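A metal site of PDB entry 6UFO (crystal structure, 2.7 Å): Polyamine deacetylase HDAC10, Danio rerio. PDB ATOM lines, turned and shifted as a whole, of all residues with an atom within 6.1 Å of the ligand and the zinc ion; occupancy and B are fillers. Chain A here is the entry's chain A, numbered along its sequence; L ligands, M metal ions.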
ATOM      1  N   ALA A  24      12.803 -23.355 -15.173  1.00  0.00           N
ATOM      2  CA  ALA A  24      11.726 -24.005 -15.903  1.00  0.00           C
ATOM      3  C   ALA A  24      11.023 -23.083 -16.889  1.00  0.00           C
ATOM      4  O   ALA A  24      10.230 -23.569 -17.703  1.00  0.00           O
ATOM      5  CB  ALA A  24      10.700 -24.580 -14.925  1.00  0.00           C
ATOM      6  N   CYS A  25      11.285 -21.773 -16.833  1.00  0.00           N
ATOM      7  CA  CYS A  25      10.586 -20.813 -17.680  1.00  0.00           C
ATOM      8  C   CYS A  25      11.499 -20.008 -18.596  1.00  0.00           C
ATOM      9  O   CYS A  25      10.981 -19.337 -19.497  1.00  0.00           O
ATOM     10  CB  CYS A  25       9.778 -19.833 -16.809  1.00  0.00           C
ATOM     11  SG  CYS A  25       8.253 -20.518 -16.111  1.00  0.00           S
ATOM     12  N   ILE A  27      13.196 -20.694 -21.056  1.00  0.00           N
ATOM     13  CA  ILE A  27      13.227 -21.065 -22.475  1.00  0.00           C
ATOM     14  C   ILE A  27      12.130 -20.376 -23.279  1.00  0.00           C
ATOM     15  O   ILE A  27      12.193 -20.372 -24.505  1.00  0.00           O
ATOM     16  CB  ILE A  27      13.105 -22.587 -22.650  1.00  0.00           C
ATOM     17  CG1 ILE A  27      11.862 -23.113 -21.942  1.00  0.00           C
ATOM     18  CG2 ILE A  27      14.363 -23.281 -22.149  1.00  0.00           C
ATOM     19  CD1 ILE A  27      11.356 -24.429 -22.486  1.00  0.00           C
ATOM     20  N   ASN A  93       1.552 -23.518 -12.054  1.00  0.00           N
ATOM     21  CA  ASN A  93       2.628 -24.455 -12.367  1.00  0.00           C
ATOM     22  C   ASN A  93       3.319 -24.024 -13.664  1.00  0.00           C
ATOM     23  O   ASN A  93       2.718 -24.051 -14.737  1.00  0.00           O
ATOM     24  CB  ASN A  93       2.085 -25.873 -12.487  1.00  0.00           C
ATOM     25  CG  ASN A  93       3.193 -26.916 -12.578  1.00  0.00           C
ATOM     26  OD1 ASN A  93       3.415 -27.504 -13.630  1.00  0.00           O
ATOM     27  ND2 ASN A  93       3.878 -27.135 -11.468  1.00  0.00           N
ATOM     28  N   ASP A  94       4.594 -23.637 -13.550  1.00  0.00           N
ATOM     29  CA  ASP A  94       5.463 -23.343 -14.685  1.00  0.00           C
ATOM     30  C   ASP A  94       4.887 -22.252 -15.585  1.00  0.00           C
ATOM     31  O   ASP A  94       4.631 -22.453 -16.776  1.00  0.00           O
ATOM     32  CB  ASP A  94       5.759 -24.623 -15.481  1.00  0.00           C
ATOM     33  CG  ASP A  94       6.737 -25.539 -14.772  1.00  0.00           C
ATOM     34  OD1 ASP A  94       7.264 -25.139 -13.710  1.00  0.00           O
ATOM     35  OD2 ASP A  94       6.994 -26.648 -15.279  1.00  0.00           O
ATOM     36  N   PRO A 134       1.404 -18.956 -25.515  1.00  0.00           N
ATOM     37  CA  PRO A 134       0.609 -20.100 -25.987  1.00  0.00           C
ATOM     38  C   PRO A 134      -0.624 -20.331 -25.131  1.00  0.00           C
ATOM     39  O   PRO A 134      -0.886 -19.563 -24.209  1.00  0.00           O
ATOM     40  CB  PRO A 134       1.603 -21.262 -25.898  1.00  0.00           C
ATOM     41  CG  PRO A 134       2.546 -20.863 -24.822  1.00  0.00           C
ATOM     42  CD  PRO A 134       2.704 -19.372 -24.962  1.00  0.00           C
ATOM     43  N   GLY A 135      -1.380 -21.395 -25.416  1.00  0.00           N
ATOM     44  CA  GLY A 135      -2.657 -21.543 -24.739  1.00  0.00           C
ATOM     45  C   GLY A 135      -3.110 -22.935 -24.331  1.00  0.00           C
ATOM     46  O   GLY A 135      -3.896 -23.057 -23.389  1.00  0.00           O
ATOM     47  N   HIS A 136      -2.625 -23.981 -25.007  1.00  0.00           N
ATOM     48  CA  HIS A 136      -3.282 -25.286 -24.871  1.00  0.00           C
ATOM     49  C   HIS A 136      -3.152 -25.895 -23.476  1.00  0.00           C
ATOM     50  O   HIS A 136      -3.813 -26.889 -23.201  1.00  0.00           O
ATOM     51  CB  HIS A 136      -2.763 -26.250 -25.950  1.00  0.00           C
ATOM     52  CG  HIS A 136      -1.417 -26.840 -25.680  1.00  0.00           C
ATOM     53  ND1 HIS A 136      -0.877 -27.829 -26.479  1.00  0.00           N
ATOM     54  CD2 HIS A 136      -0.502 -26.598 -24.714  1.00  0.00           C
ATOM     55  CE1 HIS A 136       0.317 -28.166 -26.016  1.00  0.00           C
ATOM     56  NE2 HIS A 136       0.569 -27.431 -24.944  1.00  0.00           N
ATOM     57  N   HIS A 137      -2.326 -25.310 -22.598  1.00  0.00           N
ATOM     58  CA  HIS A 137      -2.261 -25.754 -21.212  1.00  0.00           C
ATOM     59  C   HIS A 137      -3.201 -24.989 -20.303  1.00  0.00           C
ATOM     60  O   HIS A 137      -3.439 -25.424 -19.167  1.00  0.00           O
ATOM     61  CB  HIS A 137      -0.826 -25.611 -20.673  1.00  0.00           C
ATOM     62  CG  HIS A 137       0.148 -26.577 -21.281  1.00  0.00           C
ATOM     63  ND1 HIS A 137      -0.166 -27.889 -21.546  1.00  0.00           N
ATOM     64  CD2 HIS A 137       1.436 -26.417 -21.660  1.00  0.00           C
ATOM     65  CE1 HIS A 137       0.882 -28.492 -22.064  1.00  0.00           C
ATOM     66  NE2 HIS A 137       1.872 -27.627 -22.142  1.00  0.00           N
ATOM     67  N   GLY A 145       1.831 -23.878 -17.714  1.00  0.00           N
ATOM     68  CA  GLY A 145       2.789 -24.121 -18.775  1.00  0.00           C
ATOM     69  C   GLY A 145       2.916 -23.011 -19.797  1.00  0.00           C
ATOM     70  O   GLY A 145       2.676 -23.231 -20.993  1.00  0.00           O
ATOM     71  N   PHE A 146       3.269 -21.811 -19.330  1.00  0.00           N
ATOM     72  CA  PHE A 146       3.448 -20.603 -20.144  1.00  0.00           C
ATOM     73  C   PHE A 146       2.158 -20.097 -20.760  1.00  0.00           C
ATOM     74  O   PHE A 146       2.183 -19.139 -21.541  1.00  0.00           O
ATOM     75  CB  PHE A 146       4.471 -20.811 -21.276  1.00  0.00           C
ATOM     76  CG  PHE A 146       5.760 -21.456 -20.841  1.00  0.00           C
ATOM     77  CD1 PHE A 146       6.265 -21.261 -19.566  1.00  0.00           C
ATOM     78  CD2 PHE A 146       6.470 -22.258 -21.730  1.00  0.00           C
ATOM     79  CE1 PHE A 146       7.444 -21.865 -19.175  1.00  0.00           C
ATOM     80  CE2 PHE A 146       7.653 -22.853 -21.341  1.00  0.00           C
ATOM     81  CZ  PHE A 146       8.145 -22.653 -20.066  1.00  0.00           C
ATOM     82  N   CYS A 147       1.019 -20.707 -20.438  1.00  0.00           N
ATOM     83  CA  CYS A 147      -0.260 -20.367 -21.055  1.00  0.00           C
ATOM     84  C   CYS A 147      -1.133 -19.592 -20.080  1.00  0.00           C
ATOM     85  O   CYS A 147      -1.251 -19.965 -18.907  1.00  0.00           O
ATOM     86  CB  CYS A 147      -0.992 -21.622 -21.531  1.00  0.00           C
ATOM     87  SG  CYS A 147      -0.019 -22.689 -22.600  1.00  0.00           S
ATOM     88  N   ASP A 174       1.989 -30.420 -30.722  1.00  0.00           N
ATOM     89  CA  ASP A 174       2.966 -29.955 -29.749  1.00  0.00           C
ATOM     90  C   ASP A 174       3.487 -31.149 -28.950  1.00  0.00           C
ATOM     91  O   ASP A 174       2.805 -32.163 -28.794  1.00  0.00           O
ATOM     92  CB  ASP A 174       2.334 -28.923 -28.823  1.00  0.00           C
ATOM     93  CG  ASP A 174       3.315 -28.328 -27.830  1.00  0.00           C
ATOM     94  OD1 ASP A 174       3.878 -27.253 -28.110  1.00  0.00           O
ATOM     95  OD2 ASP A 174       3.502 -28.934 -26.759  1.00  0.00           O
ATOM     96  N   VAL A 175       4.715 -31.033 -28.434  1.00  0.00           N
ATOM     97  CA  VAL A 175       5.320 -32.147 -27.722  1.00  0.00           C
ATOM     98  C   VAL A 175       4.731 -32.332 -26.325  1.00  0.00           C
ATOM     99  O   VAL A 175       4.949 -33.385 -25.716  1.00  0.00           O
ATOM    100  CB  VAL A 175       6.853 -31.981 -27.627  1.00  0.00           C
ATOM    101  CG1 VAL A 175       7.239 -31.130 -26.422  1.00  0.00           C
ATOM    102  CG2 VAL A 175       7.529 -33.343 -27.582  1.00  0.00           C
ATOM    103  N   HIS A 176       4.006 -31.351 -25.812  1.00  0.00           N
ATOM    104  CA  HIS A 176       3.332 -31.466 -24.524  1.00  0.00           C
ATOM    105  C   HIS A 176       1.848 -31.765 -24.734  1.00  0.00           C
ATOM    106  O   HIS A 176       1.269 -31.433 -25.769  1.00  0.00           O
ATOM    107  CB  HIS A 176       3.479 -30.176 -23.706  1.00  0.00           C
ATOM    108  CG  HIS A 176       4.895 -29.804 -23.434  1.00  0.00           C
ATOM    109  ND1 HIS A 176       5.664 -29.069 -24.316  1.00  0.00           N
ATOM    110  CD2 HIS A 176       5.685 -30.034 -22.360  1.00  0.00           C
ATOM    111  CE1 HIS A 176       6.858 -28.887 -23.807  1.00  0.00           C
ATOM    112  NE2 HIS A 176       6.909 -29.465 -22.617  1.00  0.00           N
ATOM    113  N   HIS A 177       1.253 -32.400 -23.730  1.00  0.00           N
ATOM    114  CA  HIS A 177      -0.174 -32.713 -23.779  1.00  0.00           C
ATOM    115  C   HIS A 177      -0.977 -31.463 -23.447  1.00  0.00           C
ATOM    116  O   HIS A 177      -0.806 -30.879 -22.374  1.00  0.00           O
ATOM    117  CB  HIS A 177      -0.519 -33.847 -22.809  1.00  0.00           C
ATOM    118  CG  HIS A 177      -1.974 -34.176 -22.774  1.00  0.00           C
ATOM    119  ND1 HIS A 177      -2.694 -34.257 -21.598  1.00  0.00           N
ATOM    120  CD2 HIS A 177      -2.854 -34.454 -23.764  1.00  0.00           C
ATOM    121  CE1 HIS A 177      -3.952 -34.573 -21.866  1.00  0.00           C
ATOM    122  NE2 HIS A 177      -4.069 -34.697 -23.176  1.00  0.00           N
ATOM    123  N   TRP A 205       6.465 -33.851 -17.735  1.00  0.00           N
ATOM    124  CA  TRP A 205       5.500 -32.808 -17.430  1.00  0.00           C
ATOM    125  C   TRP A 205       4.369 -32.818 -18.461  1.00  0.00           C
ATOM    126  O   TRP A 205       4.625 -33.018 -19.661  1.00  0.00           O
ATOM    127  CB  TRP A 205       6.196 -31.446 -17.413  1.00  0.00           C
ATOM    128  CG  TRP A 205       5.391 -30.342 -16.814  1.00  0.00           C
ATOM    129  CD1 TRP A 205       5.393 -29.947 -15.508  1.00  0.00           C
ATOM    130  CD2 TRP A 205       4.454 -29.505 -17.486  1.00  0.00           C
ATOM    131  NE1 TRP A 205       4.514 -28.903 -15.327  1.00  0.00           N
ATOM    132  CE2 TRP A 205       3.927 -28.609 -16.537  1.00  0.00           C
ATOM    133  CE3 TRP A 205       4.011 -29.415 -18.815  1.00  0.00           C
ATOM    134  CZ2 TRP A 205       2.973 -27.649 -16.858  1.00  0.00           C
ATOM    135  CZ3 TRP A 205       3.070 -28.459 -19.135  1.00  0.00           C
ATOM    136  CH2 TRP A 205       2.558 -27.579 -18.163  1.00  0.00           C
ATOM    137  N   GLY A 265       2.656 -26.731 -32.040  1.00  0.00           N
ATOM    138  CA  GLY A 265       3.868 -26.584 -31.264  1.00  0.00           C
ATOM    139  C   GLY A 265       5.006 -27.339 -31.937  1.00  0.00           C
ATOM    140  O   GLY A 265       4.876 -28.521 -32.252  1.00  0.00           O
ATOM    141  N   ASP A 267       8.074 -27.756 -30.668  1.00  0.00           N
ATOM    142  CA  ASP A 267       9.010 -28.408 -29.761  1.00  0.00           C
ATOM    143  C   ASP A 267       9.064 -29.914 -29.957  1.00  0.00           C
ATOM    144  O   ASP A 267       9.833 -30.588 -29.262  1.00  0.00           O
ATOM    145  CB  ASP A 267       8.662 -28.082 -28.305  1.00  0.00           C
ATOM    146  CG  ASP A 267       7.174 -28.191 -28.026  1.00  0.00           C
ATOM    147  OD1 ASP A 267       6.423 -28.644 -28.918  1.00  0.00           O
ATOM    148  OD2 ASP A 267       6.761 -27.826 -26.903  1.00  0.00           O
ATOM    149  N   GLU A 274      13.276 -29.272 -24.946  1.00  0.00           N
ATOM    150  CA  GLU A 274      12.159 -29.744 -24.130  1.00  0.00           C
ATOM    151  C   GLU A 274      11.515 -31.007 -24.692  1.00  0.00           C
ATOM    152  O   GLU A 274      11.042 -31.842 -23.907  1.00  0.00           O
ATOM    153  CB  GLU A 274      11.105 -28.634 -24.012  1.00  0.00           C
ATOM    154  CG  GLU A 274      10.080 -28.869 -22.918  1.00  0.00           C
ATOM    155  CD  GLU A 274      10.641 -28.625 -21.530  1.00  0.00           C
ATOM    156  OE1 GLU A 274      10.110 -29.223 -20.568  1.00  0.00           O
ATOM    157  OE2 GLU A 274      11.581 -27.826 -21.401  1.00  0.00           O
ATOM    158  N   LEU A 303       0.202 -21.105 -33.409  1.00  0.00           N
ATOM    159  CA  LEU A 303       1.511 -21.396 -32.844  1.00  0.00           C
ATOM    160  C   LEU A 303       1.398 -21.688 -31.351  1.00  0.00           C
ATOM    161  O   LEU A 303       0.652 -21.032 -30.629  1.00  0.00           O
ATOM    162  CB  LEU A 303       2.451 -20.209 -33.099  1.00  0.00           C
ATOM    163  CG  LEU A 303       3.952 -20.300 -32.809  1.00  0.00           C
ATOM    164  CD1 LEU A 303       4.275 -19.874 -31.376  1.00  0.00           C
ATOM    165  CD2 LEU A 303       4.491 -21.690 -33.094  1.00  0.00           C
ATOM    166  N   GLU A 304       2.147 -22.701 -30.902  1.00  0.00           N
ATOM    167  CA  GLU A 304       2.123 -23.097 -29.495  1.00  0.00           C
ATOM    168  C   GLU A 304       3.524 -23.090 -28.913  1.00  0.00           C
ATOM    169  O   GLU A 304       3.990 -22.061 -28.399  1.00  0.00           O
ATOM    170  CB  GLU A 304       1.487 -24.486 -29.359  1.00  0.00           C
ATOM    171  CG  GLU A 304       0.009 -24.549 -29.735  1.00  0.00           C
ATOM    172  CD  GLU A 304      -0.928 -24.086 -28.619  1.00  0.00           C
ATOM    173  OE1 GLU A 304      -0.449 -23.457 -27.655  1.00  0.00           O
ATOM    174  OE2 GLU A 304      -2.140 -24.345 -28.711  1.00  0.00           O
ATOM    175  N   GLY A 305       4.220 -24.229 -28.982  1.00  0.00           N
ATOM    176  CA  GLY A 305       5.568 -24.354 -28.470  1.00  0.00           C
ATOM    177  C   GLY A 305       6.623 -24.314 -29.562  1.00  0.00           C
ATOM    178  O   GLY A 305       6.351 -24.046 -30.733  1.00  0.00           O
ATOM    179  N   GLY A 306       7.851 -24.614 -29.157  1.00  0.00           N
ATOM    180  CA  GLY A 306       9.003 -24.557 -30.046  1.00  0.00           C
ATOM    181  C   GLY A 306      10.078 -23.638 -29.507  1.00  0.00           C
ATOM    182  O   GLY A 306       9.917 -22.413 -29.523  1.00  0.00           O
ATOM    183  N   TYR A 307      11.193 -24.212 -29.030  1.00  0.00           N
ATOM    184  CA  TYR A 307      12.172 -23.457 -28.270  1.00  0.00           C
ATOM    185  C   TYR A 307      13.583 -23.485 -28.827  1.00  0.00           C
ATOM    186  O   TYR A 307      14.449 -22.774 -28.304  1.00  0.00           O
ATOM    187  CB  TYR A 307      12.185 -23.941 -26.812  1.00  0.00           C
ATOM    188  CG  TYR A 307      10.815 -23.948 -26.193  1.00  0.00           C
ATOM    189  CD1 TYR A 307      10.240 -22.771 -25.737  1.00  0.00           C
ATOM    190  CD2 TYR A 307      10.085 -25.119 -26.092  1.00  0.00           C
ATOM    191  CE1 TYR A 307       8.981 -22.761 -25.178  1.00  0.00           C
ATOM    192  CE2 TYR A 307       8.819 -25.127 -25.532  1.00  0.00           C
ATOM    193  CZ  TYR A 307       8.271 -23.939 -25.082  1.00  0.00           C
ATOM    194  OH  TYR A 307       7.019 -23.932 -24.529  1.00  0.00           O
HETATM  195  C1  LIG L   1       6.012 -26.454 -19.519  1.00  0.00           C
HETATM  196  C2  LIG L   1       7.228 -27.352 -19.118  1.00  0.00           C
HETATM  197  C3  LIG L   1       9.440 -27.351 -17.961  1.00  0.00           C
HETATM  198  C4  LIG L   1       9.526 -28.546 -16.964  1.00  0.00           C
HETATM  199  C5  LIG L   1      10.199 -28.197 -15.600  1.00  0.00           C
HETATM  200  C6  LIG L   1       1.857 -24.678 -25.924  1.00  0.00           C
HETATM  201  C7  LIG L   1       4.065 -24.617 -25.261  1.00  0.00           C
HETATM  202  C8  LIG L   1       4.527 -25.871 -24.404  1.00  0.00           C
HETATM  203  C9  LIG L   1       4.511 -25.301 -22.971  1.00  0.00           C
HETATM  204  C10 LIG L   1       4.884 -26.346 -21.893  1.00  0.00           C
HETATM  205  C11 LIG L   1       6.064 -25.920 -20.977  1.00  0.00           C
HETATM  206  N1  LIG L   1       8.064 -26.759 -18.034  1.00  0.00           N
HETATM  207  N2  LIG L   1       9.303 -28.480 -14.453  1.00  0.00           N
HETATM  208  O1  LIG L   1       2.749 -24.327 -24.911  1.00  0.00           O
HETATM  209  O2  LIG L   1       5.775 -26.289 -24.826  1.00  0.00           O
HETATM  210  O3  LIG L   1       3.604 -26.911 -24.493  1.00  0.00           O
HETATM  211 ZN    ZN M   1       5.038 -27.772 -25.952  1.00  0.00          ZN
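O3 of the ligand lies close to NE2 of His 136.
O3 of the ligand sits close to NE2 of His 137 (3.0 Å).
OD2 of Asp 94 is in salt-bridge range of N1 of the ligand, 3.0 Å away.
The side-chain hydroxyl (OH) of Tyr 307 sits close to an oxygen (O2) of the ligand (2.7 Å).
The backbone carbonyl oxygen of Asp 94 sits close to the backbone NH of Gly 145, 3.3 Å away.
The side-chain sulfur (SG) of Cys 147 sits at hydrogen-bond distance from the backbone NH (N) of His 137 (3.5 Å).
OD1 of Asp 174 sits close to N of Gly 305.
OD1 of Asp 267 lies within hydrogen-bond range of N of Val 175, 3.0 Å away.
A ring nitrogen (NE2) of His 137 lies close to a ring nitrogen (NE2) of His 136, at 3.1 Å.
The side-chain amide oxygen (OD1) of Asn 93 is in hydrogen-bond range of the indole nitrogen (NE1) of Trp 205 (2.5 Å).
The backbone carbonyl oxygen (O) of Pro 134 lies close to the side-chain sulfur (SG) of Cys 147.
The backbone carbonyl oxygen (O) of Asp 94 is in hydrogen-bond range of the backbone NH (N) of Phe 146 (3.0 Å).
Merely in contact with the ligand: Ala 24, Pro 134, Gly 145, Phe 146, Cys 147, Trp 205, Glu 274, Glu 304 and Gly 305.
16 residues have an atom within 4 Å of the ligand: Ala 24, Asp 94, Pro 134, His 136, His 137, Gly 145, Phe 146, Cys 147, Asp 174, His 176, Trp 205, Asp 267, Glu 274, Glu 304, Gly 305 and Tyr 307.
The zinc ion is bound by the side-chain carboxylate (OD2) of Asp 267 (2.0 Å), an oxygen (O2) of the ligand (2.0 Å), the side-chain carboxylate (OD2) of Asp 174 (2.1 Å), a ring nitrogen (ND1) of His 176 (2.2 Å), an oxygen (O3) of the ligand (2.2 Å) and the side-chain carboxylate (OD1) of Asp 174 (2.5 Å).
The zinc ion has six donor atoms within binding distance.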
